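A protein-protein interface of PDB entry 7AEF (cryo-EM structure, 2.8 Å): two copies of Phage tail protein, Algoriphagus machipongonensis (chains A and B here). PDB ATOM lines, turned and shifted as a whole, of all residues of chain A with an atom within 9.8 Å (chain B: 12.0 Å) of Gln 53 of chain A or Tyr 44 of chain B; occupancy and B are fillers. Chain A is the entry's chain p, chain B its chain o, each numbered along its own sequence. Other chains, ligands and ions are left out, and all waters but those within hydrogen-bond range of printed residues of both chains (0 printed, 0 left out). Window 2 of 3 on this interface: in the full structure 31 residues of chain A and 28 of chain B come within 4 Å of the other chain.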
ATOM      1  N   ASP A  28     -18.807  -2.714  12.846  1.00  0.00           N
ATOM      2  CA  ASP A  28     -20.234  -2.399  13.040  1.00  0.00           C
ATOM      3  C   ASP A  28     -21.227  -3.419  12.460  1.00  0.00           C
ATOM      4  O   ASP A  28     -20.911  -4.139  11.514  1.00  0.00           O
ATOM      5  CB  ASP A  28     -20.549  -1.060  12.390  1.00  0.00           C
ATOM      6  CG  ASP A  28     -19.853   0.119  13.012  1.00  0.00           C
ATOM      7  OD1 ASP A  28     -19.845   0.229  14.210  1.00  0.00           O
ATOM      8  OD2 ASP A  28     -19.324   0.919  12.271  1.00  0.00           O
ATOM      9  N   LEU A  29     -22.445  -3.430  13.016  1.00  0.00           N
ATOM     10  CA  LEU A  29     -23.586  -4.247  12.562  1.00  0.00           C
ATOM     11  C   LEU A  29     -24.819  -3.345  12.386  1.00  0.00           C
ATOM     12  O   LEU A  29     -25.100  -2.545  13.277  1.00  0.00           O
ATOM     13  CB  LEU A  29     -23.909  -5.306  13.631  1.00  0.00           C
ATOM     14  CG  LEU A  29     -22.785  -6.320  14.000  1.00  0.00           C
ATOM     15  CD1 LEU A  29     -23.185  -7.099  15.218  1.00  0.00           C
ATOM     16  CD2 LEU A  29     -22.553  -7.264  12.882  1.00  0.00           C
ATOM     17  N   GLU A  30     -25.590  -3.485  11.296  1.00  0.00           N
ATOM     18  CA  GLU A  30     -26.774  -2.621  11.112  1.00  0.00           C
ATOM     19  C   GLU A  30     -27.991  -3.296  10.443  1.00  0.00           C
ATOM     20  O   GLU A  30     -27.853  -4.069   9.498  1.00  0.00           O
ATOM     21  CB  GLU A  30     -26.356  -1.394  10.311  1.00  0.00           C
ATOM     22  CG  GLU A  30     -27.416  -0.350  10.107  1.00  0.00           C
ATOM     23  CD  GLU A  30     -26.888   0.838   9.372  1.00  0.00           C
ATOM     24  OE1 GLU A  30     -25.709   0.908   9.169  1.00  0.00           O
ATOM     25  OE2 GLU A  30     -27.666   1.655   8.963  1.00  0.00           O
ATOM     26  N   THR A  31     -29.200  -2.989  10.938  1.00  0.00           N
ATOM     27  CA  THR A  31     -30.457  -3.530  10.383  1.00  0.00           C
ATOM     28  C   THR A  31     -31.443  -2.422   9.979  1.00  0.00           C
ATOM     29  O   THR A  31     -31.624  -1.452  10.714  1.00  0.00           O
ATOM     30  CB  THR A  31     -31.147  -4.479  11.401  1.00  0.00           C
ATOM     31  OG1 THR A  31     -30.261  -5.540  11.733  1.00  0.00           O
ATOM     32  CG2 THR A  31     -32.406  -5.103  10.805  1.00  0.00           C
ATOM     33  N   GLU A  32     -32.092  -2.590   8.822  1.00  0.00           N
ATOM     34  CA  GLU A  32     -33.116  -1.669   8.308  1.00  0.00           C
ATOM     35  C   GLU A  32     -34.475  -1.813   8.992  1.00  0.00           C
ATOM     36  O   GLU A  32     -34.791  -2.858   9.564  1.00  0.00           O
ATOM     37  CB  GLU A  32     -33.322  -1.896   6.818  1.00  0.00           C
ATOM     38  CG  GLU A  32     -32.161  -1.536   5.965  1.00  0.00           C
ATOM     39  CD  GLU A  32     -31.965  -0.074   5.932  1.00  0.00           C
ATOM     40  OE1 GLU A  32     -32.937   0.625   5.858  1.00  0.00           O
ATOM     41  OE2 GLU A  32     -30.847   0.370   5.994  1.00  0.00           O
ATOM     42  N   ILE A  33     -35.286  -0.762   8.923  1.00  0.00           N
ATOM     43  CA  ILE A  33     -36.600  -0.785   9.557  1.00  0.00           C
ATOM     44  C   ILE A  33     -37.772  -0.588   8.597  1.00  0.00           C
ATOM     45  O   ILE A  33     -37.781   0.337   7.782  1.00  0.00           O
ATOM     46  CB  ILE A  33     -36.697   0.267  10.679  1.00  0.00           C
ATOM     47  CG1 ILE A  33     -35.575   0.065  11.699  1.00  0.00           C
ATOM     48  CG2 ILE A  33     -38.057   0.198  11.357  1.00  0.00           C
ATOM     49  CD1 ILE A  33     -35.594   1.063  12.835  1.00  0.00           C
ATOM     50  N   ILE A  34     -38.759  -1.470   8.709  1.00  0.00           N
ATOM     51  CA  ILE A  34     -39.970  -1.414   7.908  1.00  0.00           C
ATOM     52  C   ILE A  34     -41.118  -0.853   8.758  1.00  0.00           C
ATOM     53  O   ILE A  34     -41.399  -1.356   9.845  1.00  0.00           O
ATOM     54  CB  ILE A  34     -40.317  -2.809   7.371  1.00  0.00           C
ATOM     55  CG1 ILE A  34     -39.152  -3.311   6.499  1.00  0.00           C
ATOM     56  CG2 ILE A  34     -41.629  -2.747   6.583  1.00  0.00           C
ATOM     57  CD1 ILE A  34     -39.212  -4.758   6.146  1.00  0.00           C
ATOM     58  N   PRO A  50     -38.003  -5.289  11.907  1.00  0.00           N
ATOM     59  CA  PRO A  50     -36.748  -5.524  11.196  1.00  0.00           C
ATOM     60  C   PRO A  50     -36.849  -5.892   9.716  1.00  0.00           C
ATOM     61  O   PRO A  50     -37.657  -6.735   9.328  1.00  0.00           O
ATOM     62  CB  PRO A  50     -36.182  -6.730  11.947  1.00  0.00           C
ATOM     63  CG  PRO A  50     -36.776  -6.668  13.297  1.00  0.00           C
ATOM     64  CD  PRO A  50     -38.159  -6.145  13.100  1.00  0.00           C
ATOM     65  N   GLY A  51     -35.951  -5.300   8.947  1.00  0.00           N
ATOM     66  CA  GLY A  51     -35.707  -5.470   7.520  1.00  0.00           C
ATOM     67  C   GLY A  51     -34.410  -6.244   7.256  1.00  0.00           C
ATOM     68  O   GLY A  51     -34.009  -7.112   8.032  1.00  0.00           O
ATOM     69  N   MET A  52     -33.795  -5.958   6.107  1.00  0.00           N
ATOM     70  CA  MET A  52     -32.545  -6.575   5.659  1.00  0.00           C
ATOM     71  C   MET A  52     -31.333  -6.024   6.421  1.00  0.00           C
ATOM     72  O   MET A  52     -31.396  -4.938   7.006  1.00  0.00           O
ATOM     73  CB  MET A  52     -32.379  -6.396   4.164  1.00  0.00           C
ATOM     74  CG  MET A  52     -33.414  -7.167   3.353  1.00  0.00           C
ATOM     75  SD  MET A  52     -33.257  -6.973   1.574  1.00  0.00           S
ATOM     76  CE  MET A  52     -31.811  -7.959   1.218  1.00  0.00           C
ATOM     77  N   GLN A  53     -30.229  -6.784   6.433  1.00  0.00           N
ATOM     78  CA  GLN A  53     -29.020  -6.387   7.164  1.00  0.00           C
ATOM     79  C   GLN A  53     -27.837  -5.907   6.313  1.00  0.00           C
ATOM     80  O   GLN A  53     -27.682  -6.298   5.156  1.00  0.00           O
ATOM     81  CB  GLN A  53     -28.579  -7.554   8.028  1.00  0.00           C
ATOM     82  CG  GLN A  53     -29.624  -7.949   9.047  1.00  0.00           C
ATOM     83  CD  GLN A  53     -29.197  -9.088   9.913  1.00  0.00           C
ATOM     84  OE1 GLN A  53     -28.229  -9.786   9.597  1.00  0.00           O
ATOM     85  NE2 GLN A  53     -29.909  -9.301  11.004  1.00  0.00           N
ATOM     86  N   LYS A  54     -26.999  -5.066   6.934  1.00  0.00           N
ATOM     87  CA  LYS A  54     -25.770  -4.490   6.378  1.00  0.00           C
ATOM     88  C   LYS A  54     -24.531  -4.648   7.253  1.00  0.00           C
ATOM     89  O   LYS A  54     -24.611  -4.789   8.482  1.00  0.00           O
ATOM     90  CB  LYS A  54     -25.936  -3.001   6.156  1.00  0.00           C
ATOM     91  CG  LYS A  54     -26.930  -2.604   5.126  1.00  0.00           C
ATOM     92  CD  LYS A  54     -27.124  -1.095   5.119  1.00  0.00           C
ATOM     93  CE  LYS A  54     -28.052  -0.668   6.260  1.00  0.00           C
ATOM     94  NZ  LYS A  54     -28.402   0.785   6.221  1.00  0.00           N
ATOM     95  N   PHE A  55     -23.367  -4.557   6.606  1.00  0.00           N
ATOM     96  CA  PHE A  55     -22.086  -4.527   7.301  1.00  0.00           C
ATOM     97  C   PHE A  55     -21.239  -3.363   6.794  1.00  0.00           C
ATOM     98  O   PHE A  55     -21.332  -2.999   5.625  1.00  0.00           O
ATOM     99  CB  PHE A  55     -21.328  -5.823   7.086  1.00  0.00           C
ATOM    100  CG  PHE A  55     -22.042  -7.004   7.593  1.00  0.00           C
ATOM    101  CD1 PHE A  55     -22.767  -7.796   6.737  1.00  0.00           C
ATOM    102  CD2 PHE A  55     -22.040  -7.302   8.932  1.00  0.00           C
ATOM    103  CE1 PHE A  55     -23.470  -8.856   7.205  1.00  0.00           C
ATOM    104  CE2 PHE A  55     -22.747  -8.366   9.399  1.00  0.00           C
ATOM    105  CZ  PHE A  55     -23.465  -9.140   8.538  1.00  0.00           C
ATOM    106  N   SER A  56     -20.397  -2.802   7.657  1.00  0.00           N
ATOM    107  CA  SER A  56     -19.463  -1.734   7.268  1.00  0.00           C
ATOM    108  C   SER A  56     -18.123  -2.285   6.792  1.00  0.00           C
ATOM    109  O   SER A  56     -17.736  -3.397   7.162  1.00  0.00           O
ATOM    110  CB  SER A  56     -19.208  -0.787   8.425  1.00  0.00           C
ATOM    111  OG  SER A  56     -20.366  -0.093   8.794  1.00  0.00           O
ATOM    112  N   LYS A 106     -15.804 -13.014   7.982  1.00  0.00           N
ATOM    113  CA  LYS A 106     -15.935 -13.917   6.832  1.00  0.00           C
ATOM    114  C   LYS A 106     -15.663 -13.284   5.442  1.00  0.00           C
ATOM    115  O   LYS A 106     -16.228 -12.240   5.114  1.00  0.00           O
ATOM    116  CB  LYS A 106     -17.362 -14.463   6.883  1.00  0.00           C
ATOM    117  CG  LYS A 106     -17.741 -15.485   5.852  1.00  0.00           C
ATOM    118  CD  LYS A 106     -19.128 -16.089   6.149  1.00  0.00           C
ATOM    119  CE  LYS A 106     -20.258 -15.061   5.920  1.00  0.00           C
ATOM    120  NZ  LYS A 106     -21.596 -15.658   6.031  1.00  0.00           N
ATOM    121  N   HIS A 134     -16.323  -7.322   3.276  1.00  0.00           N
ATOM    122  CA  HIS A 134     -16.512  -8.657   3.854  1.00  0.00           C
ATOM    123  C   HIS A 134     -17.981  -9.044   3.829  1.00  0.00           C
ATOM    124  O   HIS A 134     -18.829  -8.240   3.440  1.00  0.00           O
ATOM    125  CB  HIS A 134     -15.943  -8.718   5.268  1.00  0.00           C
ATOM    126  CG  HIS A 134     -16.641  -7.878   6.231  1.00  0.00           C
ATOM    127  ND1 HIS A 134     -17.681  -8.331   7.019  1.00  0.00           N
ATOM    128  CD2 HIS A 134     -16.488  -6.581   6.508  1.00  0.00           C
ATOM    129  CE1 HIS A 134     -18.108  -7.333   7.754  1.00  0.00           C
ATOM    130  NE2 HIS A 134     -17.406  -6.255   7.443  1.00  0.00           N
ATOM    131  N   GLU A 135     -18.276 -10.285   4.207  1.00  0.00           N
ATOM    132  CA  GLU A 135     -19.644 -10.802   4.204  1.00  0.00           C
ATOM    133  C   GLU A 135     -20.229 -11.200   5.564  1.00  0.00           C
ATOM    134  O   GLU A 135     -21.167 -11.997   5.611  1.00  0.00           O
ATOM    135  CB  GLU A 135     -19.742 -11.985   3.236  1.00  0.00           C
ATOM    136  CG  GLU A 135     -19.501 -11.610   1.767  1.00  0.00           C
ATOM    137  CD  GLU A 135     -19.634 -12.763   0.804  1.00  0.00           C
ATOM    138  OE1 GLU A 135     -19.766 -13.873   1.249  1.00  0.00           O
ATOM    139  OE2 GLU A 135     -19.593 -12.531  -0.376  1.00  0.00           O
ATOM    140  N   GLY A 136     -19.707 -10.688   6.676  1.00  0.00           N
ATOM    141  CA  GLY A 136     -20.299 -11.062   7.950  1.00  0.00           C
ATOM    142  C   GLY A 136     -19.359 -11.031   9.134  1.00  0.00           C
ATOM    143  O   GLY A 136     -18.179 -11.378   9.040  1.00  0.00           O
ATOM    144  N   LEU A 137     -19.931 -10.667  10.280  1.00  0.00           N
ATOM    145  CA  LEU A 137     -19.234 -10.512  11.547  1.00  0.00           C
ATOM    146  C   LEU A 137     -19.931 -11.165  12.740  1.00  0.00           C
ATOM    147  O   LEU A 137     -21.111 -10.934  12.993  1.00  0.00           O
ATOM    148  CB  LEU A 137     -19.038  -9.000  11.818  1.00  0.00           C
ATOM    149  CG  LEU A 137     -18.497  -8.569  13.218  1.00  0.00           C
ATOM    150  CD1 LEU A 137     -17.096  -9.069  13.431  1.00  0.00           C
ATOM    151  CD2 LEU A 137     -18.521  -7.027  13.316  1.00  0.00           C
ATOM    152  N   GLU B  35     -22.611  -6.108  -6.115  1.00  0.00           N
ATOM    153  CA  GLU B  35     -23.369  -6.842  -5.088  1.00  0.00           C
ATOM    154  C   GLU B  35     -24.517  -7.692  -5.659  1.00  0.00           C
ATOM    155  O   GLU B  35     -25.157  -7.294  -6.632  1.00  0.00           O
ATOM    156  CB  GLU B  35     -23.935  -5.857  -4.074  1.00  0.00           C
ATOM    157  CG  GLU B  35     -22.900  -5.056  -3.318  1.00  0.00           C
ATOM    158  CD  GLU B  35     -23.504  -4.138  -2.300  1.00  0.00           C
ATOM    159  OE1 GLU B  35     -24.706  -4.021  -2.293  1.00  0.00           O
ATOM    160  OE2 GLU B  35     -22.779  -3.553  -1.526  1.00  0.00           O
ATOM    161  N   TYR B  36     -24.824  -8.825  -5.006  1.00  0.00           N
ATOM    162  CA  TYR B  36     -25.931  -9.702  -5.444  1.00  0.00           C
ATOM    163  C   TYR B  36     -26.647 -10.534  -4.356  1.00  0.00           C
ATOM    164  O   TYR B  36     -26.028 -11.017  -3.410  1.00  0.00           O
ATOM    165  CB  TYR B  36     -25.369 -10.672  -6.494  1.00  0.00           C
ATOM    166  CG  TYR B  36     -26.347 -11.657  -7.103  1.00  0.00           C
ATOM    167  CD1 TYR B  36     -27.128 -11.291  -8.171  1.00  0.00           C
ATOM    168  CD2 TYR B  36     -26.456 -12.933  -6.583  1.00  0.00           C
ATOM    169  CE1 TYR B  36     -28.001 -12.193  -8.722  1.00  0.00           C
ATOM    170  CE2 TYR B  36     -27.329 -13.830  -7.129  1.00  0.00           C
ATOM    171  CZ  TYR B  36     -28.096 -13.468  -8.194  1.00  0.00           C
ATOM    172  OH  TYR B  36     -28.969 -14.365  -8.749  1.00  0.00           O
ATOM    173  N   ARG B  37     -27.976 -10.692  -4.478  1.00  0.00           N
ATOM    174  CA  ARG B  37     -28.733 -11.610  -3.611  1.00  0.00           C
ATOM    175  C   ARG B  37     -29.928 -12.260  -4.312  1.00  0.00           C
ATOM    176  O   ARG B  37     -30.782 -11.567  -4.859  1.00  0.00           O
ATOM    177  CB  ARG B  37     -29.260 -10.938  -2.335  1.00  0.00           C
ATOM    178  CG  ARG B  37     -30.077 -11.898  -1.439  1.00  0.00           C
ATOM    179  CD  ARG B  37     -30.571 -11.357  -0.136  1.00  0.00           C
ATOM    180  NE  ARG B  37     -31.340 -12.419   0.564  1.00  0.00           N
ATOM    181  CZ  ARG B  37     -32.677 -12.674   0.394  1.00  0.00           C
ATOM    182  NH1 ARG B  37     -33.406 -11.901  -0.388  1.00  0.00           N
ATOM    183  NH2 ARG B  37     -33.276 -13.702   0.991  1.00  0.00           N
ATOM    184  N   HIS B  38     -30.025 -13.582  -4.273  1.00  0.00           N
ATOM    185  CA  HIS B  38     -31.185 -14.278  -4.848  1.00  0.00           C
ATOM    186  C   HIS B  38     -32.216 -14.518  -3.736  1.00  0.00           C
ATOM    187  O   HIS B  38     -31.859 -14.854  -2.629  1.00  0.00           O
ATOM    188  CB  HIS B  38     -30.828 -15.534  -5.654  1.00  0.00           C
ATOM    189  CG  HIS B  38     -30.182 -16.624  -4.864  1.00  0.00           C
ATOM    190  ND1 HIS B  38     -30.875 -17.713  -4.398  1.00  0.00           N
ATOM    191  CD2 HIS B  38     -28.903 -16.807  -4.481  1.00  0.00           C
ATOM    192  CE1 HIS B  38     -30.061 -18.503  -3.732  1.00  0.00           C
ATOM    193  NE2 HIS B  38     -28.854 -17.986  -3.785  1.00  0.00           N
ATOM    194  N   GLY B  39     -33.491 -14.321  -4.056  1.00  0.00           N
ATOM    195  CA  GLY B  39     -34.609 -14.360  -3.117  1.00  0.00           C
ATOM    196  C   GLY B  39     -34.686 -15.563  -2.175  1.00  0.00           C
ATOM    197  O   GLY B  39     -35.196 -15.431  -1.064  1.00  0.00           O
ATOM    198  N   ALA B  40     -34.204 -16.727  -2.595  1.00  0.00           N
ATOM    199  CA  ALA B  40     -34.270 -17.912  -1.749  1.00  0.00           C
ATOM    200  C   ALA B  40     -33.141 -18.044  -0.727  1.00  0.00           C
ATOM    201  O   ALA B  40     -33.127 -19.019   0.021  1.00  0.00           O
ATOM    202  CB  ALA B  40     -34.280 -19.148  -2.619  1.00  0.00           C
ATOM    203  N   SER B  41     -32.168 -17.140  -0.710  1.00  0.00           N
ATOM    204  CA  SER B  41     -31.058 -17.291   0.225  1.00  0.00           C
ATOM    205  C   SER B  41     -31.476 -17.178   1.708  1.00  0.00           C
ATOM    206  O   SER B  41     -32.232 -16.275   2.064  1.00  0.00           O
ATOM    207  CB  SER B  41     -30.002 -16.247  -0.032  1.00  0.00           C
ATOM    208  OG  SER B  41     -28.982 -16.333   0.938  1.00  0.00           O
ATOM    209  N   PRO B  42     -30.986 -18.067   2.611  1.00  0.00           N
ATOM    210  CA  PRO B  42     -31.143 -18.022   4.063  1.00  0.00           C
ATOM    211  C   PRO B  42     -30.537 -16.779   4.723  1.00  0.00           C
ATOM    212  O   PRO B  42     -30.843 -16.477   5.870  1.00  0.00           O
ATOM    213  CB  PRO B  42     -30.385 -19.268   4.524  1.00  0.00           C
ATOM    214  CG  PRO B  42     -30.394 -20.177   3.363  1.00  0.00           C
ATOM    215  CD  PRO B  42     -30.332 -19.297   2.150  1.00  0.00           C
ATOM    216  N   GLU B  43     -29.610 -16.105   4.037  1.00  0.00           N
ATOM    217  CA  GLU B  43     -29.015 -14.906   4.606  1.00  0.00           C
ATOM    218  C   GLU B  43     -29.694 -13.706   4.009  1.00  0.00           C
ATOM    219  O   GLU B  43     -30.025 -13.698   2.823  1.00  0.00           O
ATOM    220  CB  GLU B  43     -27.507 -14.837   4.384  1.00  0.00           C
ATOM    221  CG  GLU B  43     -26.722 -15.880   5.122  1.00  0.00           C
ATOM    222  CD  GLU B  43     -25.229 -15.719   4.957  1.00  0.00           C
ATOM    223  OE1 GLU B  43     -24.828 -14.968   4.107  1.00  0.00           O
ATOM    224  OE2 GLU B  43     -24.496 -16.333   5.690  1.00  0.00           O
ATOM    225  N   TYR B  44     -29.816 -12.656   4.795  1.00  0.00           N
ATOM    226  CA  TYR B  44     -30.515 -11.465   4.367  1.00  0.00           C
ATOM    227  C   TYR B  44     -29.584 -10.304   4.069  1.00  0.00           C
ATOM    228  O   TYR B  44     -29.890  -9.149   4.349  1.00  0.00           O
ATOM    229  CB  TYR B  44     -31.574 -11.134   5.403  1.00  0.00           C
ATOM    230  CG  TYR B  44     -32.455 -12.362   5.675  1.00  0.00           C
ATOM    231  CD1 TYR B  44     -32.523 -12.885   6.942  1.00  0.00           C
ATOM    232  CD2 TYR B  44     -33.124 -13.000   4.647  1.00  0.00           C
ATOM    233  CE1 TYR B  44     -33.260 -14.010   7.193  1.00  0.00           C
ATOM    234  CE2 TYR B  44     -33.852 -14.132   4.896  1.00  0.00           C
ATOM    235  CZ  TYR B  44     -33.922 -14.634   6.169  1.00  0.00           C
ATOM    236  OH  TYR B  44     -34.651 -15.763   6.428  1.00  0.00           O
ATOM    237  N   SER B  45     -28.440 -10.637   3.497  1.00  0.00           N
ATOM    238  CA  SER B  45     -27.408  -9.704   3.097  1.00  0.00           C
ATOM    239  C   SER B  45     -26.857 -10.145   1.743  1.00  0.00           C
ATOM    240  O   SER B  45     -27.204 -11.217   1.246  1.00  0.00           O
ATOM    241  CB  SER B  45     -26.322  -9.643   4.147  1.00  0.00           C
ATOM    242  OG  SER B  45     -25.655 -10.860   4.240  1.00  0.00           O
ATOM    243  N   LYS B  46     -26.041  -9.306   1.117  1.00  0.00           N
ATOM    244  CA  LYS B  46     -25.530  -9.588  -0.228  1.00  0.00           C
ATOM    245  C   LYS B  46     -24.120 -10.171  -0.309  1.00  0.00           C
ATOM    246  O   LYS B  46     -23.298  -9.975   0.584  1.00  0.00           O
ATOM    247  CB  LYS B  46     -25.595  -8.295  -1.026  1.00  0.00           C
ATOM    248  CG  LYS B  46     -27.008  -7.792  -1.213  1.00  0.00           C
ATOM    249  CD  LYS B  46     -27.056  -6.520  -1.960  1.00  0.00           C
ATOM    250  CE  LYS B  46     -28.459  -6.011  -2.090  1.00  0.00           C
ATOM    251  NZ  LYS B  46     -28.495  -4.697  -2.780  1.00  0.00           N
ATOM    252  N   ILE B  47     -23.835 -10.838  -1.430  1.00  0.00           N
ATOM    253  CA  ILE B  47     -22.502 -11.364  -1.725  1.00  0.00           C
ATOM    254  C   ILE B  47     -21.766 -10.354  -2.595  1.00  0.00           C
ATOM    255  O   ILE B  47     -22.370  -9.676  -3.427  1.00  0.00           O
ATOM    256  CB  ILE B  47     -22.527 -12.771  -2.373  1.00  0.00           C
ATOM    257  CG1 ILE B  47     -23.267 -12.766  -3.735  1.00  0.00           C
ATOM    258  CG2 ILE B  47     -23.189 -13.728  -1.388  1.00  0.00           C
ATOM    259  CD1 ILE B  47     -23.125 -14.020  -4.551  1.00  0.00           C
ATOM    260  N   LYS B  48     -20.465 -10.183  -2.356  1.00  0.00           N
ATOM    261  CA  LYS B  48     -19.700  -9.165  -3.079  1.00  0.00           C
ATOM    262  C   LYS B  48     -18.561  -9.677  -3.966  1.00  0.00           C
ATOM    263  O   LYS B  48     -17.827 -10.582  -3.576  1.00  0.00           O
ATOM    264  CB  LYS B  48     -19.118  -8.253  -2.014  1.00  0.00           C
ATOM    265  CG  LYS B  48     -20.181  -7.600  -1.182  1.00  0.00           C
ATOM    266  CD  LYS B  48     -19.640  -6.727  -0.108  1.00  0.00           C
ATOM    267  CE  LYS B  48     -20.780  -6.166   0.718  1.00  0.00           C
ATOM    268  NZ  LYS B  48     -20.303  -5.309   1.817  1.00  0.00           N
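The side-chain carboxylate (OE2) of Glu 43 of chain B is in salt-bridge range of the side-chain amino group (NZ) of Lys 106 of chain A (3.0 Å).
The backbone carbonyl oxygen (O) of Tyr 44 of chain B sits at hydrogen-bond distance from the backbone NH (N) of Gln 53 of chain A, at 3.2 Å.
The backbone NH (N) of Lys 48 of chain B is in hydrogen-bond range of the side-chain carboxylate (OE2) of Glu 135 of chain A (3.2 Å).
NH2 of Arg 37 of chain B lies within hydrogen-bond range of O of Gly 39 of chain B, at 3.3 Å.
The guanidinium group (NH2) of Arg 37 of chain B is in hydrogen-bond range of the backbone carbonyl oxygen (O) of Ser 41 of chain B.
The side-chain hydroxyl of Ser 41 of chain B lies within hydrogen-bond range of the backbone NH of Glu 43 of chain B (3.2 Å).
The backbone NH (N) of Glu 32 of chain A is in hydrogen-bond range of the backbone carbonyl oxygen (O) of Met 52 of chain A (3.0 Å).
O of Lys 106 of chain A is in hydrogen-bond range of N of Glu 135 of chain A.
ND1 of His 134 of chain A sits at hydrogen-bond distance from N of Gly 136 of chain A (3.1 Å).
Met 52 of chain A touches Arg 37 of chain B (CE to CD, 3.9 Å).
CB of Met 52 of chain A touches O of Tyr 44 of chain B, at 3.7 Å.
Ser 45 of chain B touches Gln 53 of chain A.
His 134 of chain A touches Lys 48 of chain B.
OE2 of Glu 135 of chain A touches CA of Ile 47 of chain B (3.4 Å).
Gln 53 of chain A touches just these residues of chain B: Tyr 44 and Ser 45.
Tyr 44 of chain B touches just these residues of chain A: Met 52 and Gln 53.
No residue of chain B comes within 4 Å of Thr 31 of chain A.
No residue of chain B comes within 4 Å of Glu 32 of chain A.
Of chain B, only Arg 37 (3.9 Å) and Tyr 44 (3.7 Å) come within 4 Å of Met 52 of chain A.
Phe 55 of chain A touches none of the printed residues of chain B.
Printed residues of chain B within 4 Å of Lys 106 of chain A: Glu 43.
Printed residues of chain A within 4 Å of Arg 37 of chain B: Met 52.
Printed residues of chain A within 4 Å of Glu 43 of chain B: Lys 106.
The nearest residue of chain B that does not touch Gln 53 of chain A is Lys 46 of chain B (5.3 Å).
Hydrophobic or aromatic side chains of chain B that line the printed part of chain A: Ile 47.
No position is printed for both chains.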
